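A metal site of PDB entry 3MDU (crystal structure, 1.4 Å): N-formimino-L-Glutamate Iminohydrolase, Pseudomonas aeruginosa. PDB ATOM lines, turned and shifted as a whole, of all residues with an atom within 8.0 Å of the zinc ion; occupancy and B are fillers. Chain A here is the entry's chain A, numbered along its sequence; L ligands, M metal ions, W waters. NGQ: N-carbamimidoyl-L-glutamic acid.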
ATOM      1  N   HIS A  56      -0.957  -8.885  -7.266  1.00  0.00           N
ATOM      2  CA  HIS A  56      -2.404  -9.040  -7.219  1.00  0.00           C
ATOM      3  C   HIS A  56      -2.977  -9.518  -8.544  1.00  0.00           C
ATOM      4  O   HIS A  56      -2.834  -8.850  -9.565  1.00  0.00           O
ATOM      5  CB  HIS A  56      -3.039  -7.708  -6.839  1.00  0.00           C
ATOM      6  CG  HIS A  56      -4.514  -7.785  -6.587  1.00  0.00           C
ATOM      7  ND1 HIS A  56      -5.042  -8.381  -5.468  1.00  0.00           N
ATOM      8  CD2 HIS A  56      -5.559  -7.319  -7.304  1.00  0.00           C
ATOM      9  CE1 HIS A  56      -6.365  -8.286  -5.507  1.00  0.00           C
ATOM     10  NE2 HIS A  56      -6.703  -7.643  -6.607  1.00  0.00           N
ATOM     11  N   SER A  57      -3.666 -10.657  -8.506  1.00  0.00           N
ATOM     12  CA  SER A  57      -4.209 -11.295  -9.712  1.00  0.00           C
ATOM     13  C   SER A  57      -5.520 -12.012  -9.419  1.00  0.00           C
ATOM     14  O   SER A  57      -5.635 -12.665  -8.393  1.00  0.00           O
ATOM     15  CB  SER A  57      -3.226 -12.357 -10.199  1.00  0.00           C
ATOM     16  OG  SER A  57      -3.819 -13.196 -11.190  1.00  0.00           O
ATOM     17  N   HIS A  58      -6.480 -11.912 -10.345  1.00  0.00           N
ATOM     18  CA  HIS A  58      -7.602 -12.869 -10.354  1.00  0.00           C
ATOM     19  C   HIS A  58      -7.569 -13.525 -11.731  1.00  0.00           C
ATOM     20  O   HIS A  58      -8.075 -12.967 -12.698  1.00  0.00           O
ATOM     21  CB  HIS A  58      -8.963 -12.198 -10.139  1.00  0.00           C
ATOM     22  CG  HIS A  58      -8.963 -11.185  -9.043  1.00  0.00           C
ATOM     23  ND1 HIS A  58      -8.684 -11.495  -7.726  1.00  0.00           N
ATOM     24  CD2 HIS A  58      -9.206  -9.850  -9.069  1.00  0.00           C
ATOM     25  CE1 HIS A  58      -8.739 -10.405  -6.991  1.00  0.00           C
ATOM     26  NE2 HIS A  58      -9.050  -9.388  -7.780  1.00  0.00           N
ATOM     27  N   GLN A  61     -10.136 -13.671 -14.811  1.00  0.00           N
ATOM     28  CA  GLN A  61     -10.588 -12.444 -15.456  1.00  0.00           C
ATOM     29  C   GLN A  61      -9.890 -12.173 -16.784  1.00  0.00           C
ATOM     30  O   GLN A  61     -10.415 -11.451 -17.631  1.00  0.00           O
ATOM     31  CB  GLN A  61     -10.495 -11.250 -14.495  1.00  0.00           C
ATOM     32  CG  GLN A  61     -11.515 -11.392 -13.344  1.00  0.00           C
ATOM     33  CD  GLN A  61     -11.497 -10.243 -12.352  1.00  0.00           C
ATOM     34  OE1 GLN A  61     -10.916  -9.175 -12.608  1.00  0.00           O
ATOM     35  NE2 GLN A  61     -12.132 -10.450 -11.198  1.00  0.00           N
ATOM     36  N   PHE A  78     -17.825   0.538 -12.247  1.00  0.00           N
ATOM     37  CA  PHE A  78     -17.305  -0.670 -11.640  1.00  0.00           C
ATOM     38  C   PHE A  78     -18.419  -1.663 -11.306  1.00  0.00           C
ATOM     39  O   PHE A  78     -18.239  -2.882 -11.425  1.00  0.00           O
ATOM     40  CB  PHE A  78     -16.534  -0.277 -10.371  1.00  0.00           C
ATOM     41  CG  PHE A  78     -16.207  -1.443  -9.489  1.00  0.00           C
ATOM     42  CD1 PHE A  78     -14.987  -2.094  -9.610  1.00  0.00           C
ATOM     43  CD2 PHE A  78     -17.108  -1.877  -8.541  1.00  0.00           C
ATOM     44  CE1 PHE A  78     -14.689  -3.170  -8.793  1.00  0.00           C
ATOM     45  CE2 PHE A  78     -16.814  -2.946  -7.719  1.00  0.00           C
ATOM     46  CZ  PHE A  78     -15.606  -3.600  -7.847  1.00  0.00           C
ATOM     47  N   TRP A  81     -19.857  -3.427 -14.373  1.00  0.00           N
ATOM     48  CA  TRP A  81     -18.786  -4.336 -14.763  1.00  0.00           C
ATOM     49  C   TRP A  81     -18.815  -5.609 -13.915  1.00  0.00           C
ATOM     50  O   TRP A  81     -18.623  -6.716 -14.438  1.00  0.00           O
ATOM     51  CB  TRP A  81     -17.431  -3.651 -14.633  1.00  0.00           C
ATOM     52  CG  TRP A  81     -16.267  -4.575 -14.763  1.00  0.00           C
ATOM     53  CD1 TRP A  81     -15.633  -4.939 -15.919  1.00  0.00           C
ATOM     54  CD2 TRP A  81     -15.586  -5.274 -13.708  1.00  0.00           C
ATOM     55  NE1 TRP A  81     -14.604  -5.802 -15.638  1.00  0.00           N
ATOM     56  CE2 TRP A  81     -14.544  -6.022 -14.290  1.00  0.00           C
ATOM     57  CE3 TRP A  81     -15.747  -5.317 -12.312  1.00  0.00           C
ATOM     58  CZ2 TRP A  81     -13.694  -6.821 -13.548  1.00  0.00           C
ATOM     59  CZ3 TRP A  81     -14.884  -6.117 -11.577  1.00  0.00           C
ATOM     60  CH2 TRP A  81     -13.867  -6.857 -12.191  1.00  0.00           C
ATOM     61  N   PHE A 119      -5.021 -13.858  -5.890  1.00  0.00           N
ATOM     62  CA  PHE A 119      -6.040 -13.465  -4.910  1.00  0.00           C
ATOM     63  C   PHE A 119      -7.284 -14.253  -5.326  1.00  0.00           C
ATOM     64  O   PHE A 119      -8.092 -13.837  -6.164  1.00  0.00           O
ATOM     65  CB  PHE A 119      -6.179 -11.953  -5.020  1.00  0.00           C
ATOM     66  CG  PHE A 119      -6.968 -11.273  -3.921  1.00  0.00           C
ATOM     67  CD1 PHE A 119      -8.348 -11.392  -3.845  1.00  0.00           C
ATOM     68  CD2 PHE A 119      -6.325 -10.420  -3.033  1.00  0.00           C
ATOM     69  CE1 PHE A 119      -9.057 -10.711  -2.883  1.00  0.00           C
ATOM     70  CE2 PHE A 119      -7.040  -9.732  -2.066  1.00  0.00           C
ATOM     71  CZ  PHE A 119      -8.410  -9.878  -1.983  1.00  0.00           C
ATOM     72  N   TYR A 121     -10.621 -16.385  -5.085  1.00  0.00           N
ATOM     73  CA  TYR A 121     -11.904 -16.498  -4.390  1.00  0.00           C
ATOM     74  C   TYR A 121     -12.913 -17.402  -5.099  1.00  0.00           C
ATOM     75  O   TYR A 121     -14.042 -17.532  -4.637  1.00  0.00           O
ATOM     76  CB  TYR A 121     -12.520 -15.124  -4.158  1.00  0.00           C
ATOM     77  CG  TYR A 121     -12.637 -14.272  -5.411  1.00  0.00           C
ATOM     78  CD1 TYR A 121     -13.593 -14.543  -6.372  1.00  0.00           C
ATOM     79  CD2 TYR A 121     -11.803 -13.186  -5.607  1.00  0.00           C
ATOM     80  CE1 TYR A 121     -13.702 -13.763  -7.528  1.00  0.00           C
ATOM     81  CE2 TYR A 121     -11.896 -12.400  -6.720  1.00  0.00           C
ATOM     82  CZ  TYR A 121     -12.856 -12.684  -7.686  1.00  0.00           C
ATOM     83  OH  TYR A 121     -12.946 -11.889  -8.809  1.00  0.00           O
ATOM     84  N   HIS A 206     -11.559 -10.726   1.330  1.00  0.00           N
ATOM     85  CA  HIS A 206     -11.874 -10.100   0.054  1.00  0.00           C
ATOM     86  C   HIS A 206     -11.889  -8.575   0.140  1.00  0.00           C
ATOM     87  O   HIS A 206     -11.287  -7.879  -0.681  1.00  0.00           O
ATOM     88  CB  HIS A 206     -13.196 -10.593  -0.529  1.00  0.00           C
ATOM     89  CG  HIS A 206     -13.516  -9.950  -1.831  1.00  0.00           C
ATOM     90  ND1 HIS A 206     -14.215  -8.765  -1.920  1.00  0.00           N
ATOM     91  CD2 HIS A 206     -13.173 -10.275  -3.098  1.00  0.00           C
ATOM     92  CE1 HIS A 206     -14.317  -8.409  -3.185  1.00  0.00           C
ATOM     93  NE2 HIS A 206     -13.694  -9.310  -3.923  1.00  0.00           N
ATOM     94  N   ILE A 231      -5.981  -7.648   1.389  1.00  0.00           N
ATOM     95  CA  ILE A 231      -7.370  -7.218   1.377  1.00  0.00           C
ATOM     96  C   ILE A 231      -7.572  -6.137   0.307  1.00  0.00           C
ATOM     97  O   ILE A 231      -6.704  -5.284   0.145  1.00  0.00           O
ATOM     98  CB  ILE A 231      -7.780  -6.681   2.773  1.00  0.00           C
ATOM     99  CG1 ILE A 231      -9.272  -6.381   2.841  1.00  0.00           C
ATOM    100  CG2 ILE A 231      -6.966  -5.433   3.156  1.00  0.00           C
ATOM    101  CD1 ILE A 231      -9.771  -6.116   4.271  1.00  0.00           C
ATOM    102  N   HIS A 232      -8.688  -6.174  -0.431  1.00  0.00           N
ATOM    103  CA  HIS A 232      -9.031  -5.030  -1.279  1.00  0.00           C
ATOM    104  C   HIS A 232      -9.561  -3.947  -0.350  1.00  0.00           C
ATOM    105  O   HIS A 232     -10.430  -4.232   0.490  1.00  0.00           O
ATOM    106  CB  HIS A 232     -10.228  -5.331  -2.202  1.00  0.00           C
ATOM    107  CG  HIS A 232      -9.966  -6.279  -3.344  1.00  0.00           C
ATOM    108  ND1 HIS A 232     -10.655  -7.468  -3.462  1.00  0.00           N
ATOM    109  CD2 HIS A 232      -9.215  -6.164  -4.467  1.00  0.00           C
ATOM    110  CE1 HIS A 232     -10.284  -8.076  -4.580  1.00  0.00           C
ATOM    111  NE2 HIS A 232      -9.432  -7.303  -5.218  1.00  0.00           N
ATOM    112  N   GLU A 235     -11.065   1.039  -2.812  1.00  0.00           N
ATOM    113  CA  GLU A 235     -10.953   1.149  -4.261  1.00  0.00           C
ATOM    114  C   GLU A 235     -11.896   2.172  -4.891  1.00  0.00           C
ATOM    115  O   GLU A 235     -11.485   2.979  -5.721  1.00  0.00           O
ATOM    116  CB  GLU A 235     -11.165  -0.208  -4.931  1.00  0.00           C
ATOM    117  CG  GLU A 235     -10.896  -0.175  -6.423  1.00  0.00           C
ATOM    118  CD  GLU A 235     -11.179  -1.504  -7.080  1.00  0.00           C
ATOM    119  OE1 GLU A 235     -11.656  -2.419  -6.385  1.00  0.00           O
ATOM    120  OE2 GLU A 235     -10.920  -1.633  -8.301  1.00  0.00           O
ATOM    121  N   VAL A 268      -4.721  -3.675  -1.086  1.00  0.00           N
ATOM    122  CA  VAL A 268      -4.869  -3.592  -2.535  1.00  0.00           C
ATOM    123  C   VAL A 268      -5.730  -2.409  -2.918  1.00  0.00           C
ATOM    124  O   VAL A 268      -6.819  -2.212  -2.365  1.00  0.00           O
ATOM    125  CB  VAL A 268      -5.457  -4.895  -3.132  1.00  0.00           C
ATOM    126  CG1 VAL A 268      -5.445  -4.817  -4.641  1.00  0.00           C
ATOM    127  CG2 VAL A 268      -4.649  -6.091  -2.668  1.00  0.00           C
ATOM    128  N   HIS A 269      -5.219  -1.626  -3.871  1.00  0.00           N
ATOM    129  CA  HIS A 269      -5.805  -0.370  -4.337  1.00  0.00           C
ATOM    130  C   HIS A 269      -5.546   0.778  -3.362  1.00  0.00           C
ATOM    131  O   HIS A 269      -4.727   1.656  -3.632  1.00  0.00           O
ATOM    132  CB  HIS A 269      -7.300  -0.492  -4.663  1.00  0.00           C
ATOM    133  CG  HIS A 269      -7.625  -1.639  -5.568  1.00  0.00           C
ATOM    134  ND1 HIS A 269      -7.061  -1.786  -6.821  1.00  0.00           N
ATOM    135  CD2 HIS A 269      -8.452  -2.692  -5.408  1.00  0.00           C
ATOM    136  CE1 HIS A 269      -7.532  -2.874  -7.394  1.00  0.00           C
ATOM    137  NE2 HIS A 269      -8.382  -3.445  -6.558  1.00  0.00           N
ATOM    138  N   CYS A 291      -2.794  -1.277  -8.754  1.00  0.00           N
ATOM    139  CA  CYS A 291      -3.123  -1.981  -9.990  1.00  0.00           C
ATOM    140  C   CYS A 291      -3.574  -0.929 -10.994  1.00  0.00           C
ATOM    141  O   CYS A 291      -4.766  -0.686 -11.167  1.00  0.00           O
ATOM    142  CB  CYS A 291      -4.223  -3.004  -9.714  1.00  0.00           C
ATOM    143  SG  CYS A 291      -3.780  -4.178  -8.398  1.00  0.00           S
ATOM    144  N   THR A 294      -5.838  -1.688 -14.225  1.00  0.00           N
ATOM    145  CA  THR A 294      -7.191  -2.085 -13.828  1.00  0.00           C
ATOM    146  C   THR A 294      -7.945  -0.921 -13.171  1.00  0.00           C
ATOM    147  O   THR A 294      -9.130  -0.711 -13.460  1.00  0.00           O
ATOM    148  CB  THR A 294      -7.203  -3.320 -12.923  1.00  0.00           C
ATOM    149  OG1 THR A 294      -6.857  -4.480 -13.706  1.00  0.00           O
ATOM    150  CG2 THR A 294      -8.593  -3.545 -12.320  1.00  0.00           C
ATOM    151  N   LEU A 298     -11.366   0.470 -14.587  1.00  0.00           N
ATOM    152  CA  LEU A 298     -12.583   0.445 -13.766  1.00  0.00           C
ATOM    153  C   LEU A 298     -13.022   1.835 -13.316  1.00  0.00           C
ATOM    154  O   LEU A 298     -14.067   1.978 -12.676  1.00  0.00           O
ATOM    155  CB  LEU A 298     -12.391  -0.482 -12.573  1.00  0.00           C
ATOM    156  CG  LEU A 298     -12.181  -1.956 -12.943  1.00  0.00           C
ATOM    157  CD1 LEU A 298     -11.960  -2.779 -11.695  1.00  0.00           C
ATOM    158  CD2 LEU A 298     -13.346  -2.517 -13.746  1.00  0.00           C
ATOM    159  N   SER A 319      -1.505  -6.859 -11.718  1.00  0.00           N
ATOM    160  CA  SER A 319      -2.248  -6.777 -12.969  1.00  0.00           C
ATOM    161  C   SER A 319      -3.749  -7.001 -12.806  1.00  0.00           C
ATOM    162  O   SER A 319      -4.515  -6.669 -13.703  1.00  0.00           O
ATOM    163  CB  SER A 319      -1.646  -7.687 -14.040  1.00  0.00           C
ATOM    164  OG  SER A 319      -1.735  -9.053 -13.687  1.00  0.00           O
ATOM    165  N   ASP A 320      -4.143  -7.588 -11.679  1.00  0.00           N
ATOM    166  CA  ASP A 320      -5.537  -7.608 -11.212  1.00  0.00           C
ATOM    167  C   ASP A 320      -6.563  -8.262 -12.164  1.00  0.00           C
ATOM    168  O   ASP A 320      -6.695  -9.485 -12.173  1.00  0.00           O
ATOM    169  CB  ASP A 320      -5.965  -6.192 -10.804  1.00  0.00           C
ATOM    170  CG  ASP A 320      -7.225  -6.174  -9.966  1.00  0.00           C
ATOM    171  OD1 ASP A 320      -7.741  -7.248  -9.576  1.00  0.00           O
ATOM    172  OD2 ASP A 320      -7.706  -5.060  -9.690  1.00  0.00           O
ATOM    173  N   SER A 321      -7.279  -7.442 -12.929  1.00  0.00           N
ATOM    174  CA  SER A 321      -8.261  -7.959 -13.891  1.00  0.00           C
ATOM    175  C   SER A 321      -7.596  -8.411 -15.199  1.00  0.00           C
ATOM    176  O   SER A 321      -8.244  -8.976 -16.076  1.00  0.00           O
ATOM    177  CB  SER A 321      -9.334  -6.915 -14.201  1.00  0.00           C
ATOM    178  OG  SER A 321      -8.834  -5.904 -15.071  1.00  0.00           O
HETATM  179  C   NGQ L   1     -12.885  -8.919  -7.604  1.00  0.00           C
HETATM  180  N   NGQ L   1     -12.226  -6.733  -8.452  1.00  0.00           N
HETATM  181  O1  NGQ L   1     -12.358  -9.427  -8.612  1.00  0.00           O
HETATM  182  O2  NGQ L   1     -13.180  -9.625  -6.606  1.00  0.00           O
HETATM  183  CA  NGQ L   1     -13.168  -7.421  -7.561  1.00  0.00           C
HETATM  184  CB  NGQ L   1     -14.597  -7.136  -8.041  1.00  0.00           C
HETATM  185  CD  NGQ L   1     -15.775  -6.785  -5.811  1.00  0.00           C
HETATM  186  CF  NGQ L   1     -12.101  -5.289  -8.292  1.00  0.00           C
HETATM  187  NF  NGQ L   1     -12.554  -4.724  -7.259  1.00  0.00           N
HETATM  188  CG  NGQ L   1     -15.599  -7.673  -7.027  1.00  0.00           C
HETATM  189  NG  NGQ L   1     -11.528  -4.584  -9.167  1.00  0.00           N
HETATM  190  OE1 NGQ L   1     -16.764  -6.967  -5.056  1.00  0.00           O
HETATM  191  OE2 NGQ L   1     -14.889  -5.953  -5.494  1.00  0.00           O
HETATM  192 ZN    ZN M   1      -8.669  -7.451  -7.215  1.00  0.00          ZN
HETATM  193  O   HOH W   1      -9.257  -5.653  -7.680  1.00  0.00           O
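Water W1 is bound to the zinc ion, at 1.9 Å.
A ring nitrogen (NE2) of His 58 is bound to the zinc ion.
NE2 of His 56 binds the zinc ion.
The zinc ion is bound by a ring nitrogen (NE2) of His 232, at 2.1 Å.
OD1 of Asp 320 binds the zinc ion (2.5 Å).
The zinc ion has five donor atoms within binding distance.
The backbone carbonyl oxygen of Phe 119 sits at hydrogen-bond distance from a ring nitrogen (ND1) of His 58.
N of Ser 319 is in hydrogen-bond range of O of His 56, at 3.2 Å.
A ring nitrogen (ND1) of His 232 sits at hydrogen-bond distance from the backbone carbonyl oxygen (O) of His 206 (2.9 Å).
Of the 20 residues printed, 4 come within 4 Å of the zinc ion.
The nearest printed residue that does not touch the zinc ion is His 269 (4.1 Å).
Water W1 lies within hydrogen-bond range of OD2 of Asp 320, NE2 of His 269 and NG of the ligand.
O1 of the ligand sits close to NE2 of His 58.
The side-chain carboxylate (OD2) of Asp 320 is in salt-bridge range of a nitrogen (NG) of the ligand, 3.9 Å away.
A nitrogen (NF) of the ligand is in salt-bridge range of the side-chain carboxylate of Glu 235 (2.6 Å).
An oxygen (O1) of the ligand is in hydrogen-bond range of the side-chain hydroxyl (OH) of Tyr 121 (2.5 Å).
O1 of the ligand is in hydrogen-bond range of NE2 of Gln 61, 2.8 Å away.
An oxygen (O2) of the ligand sits at hydrogen-bond distance from a ring nitrogen (NE2) of His 206.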
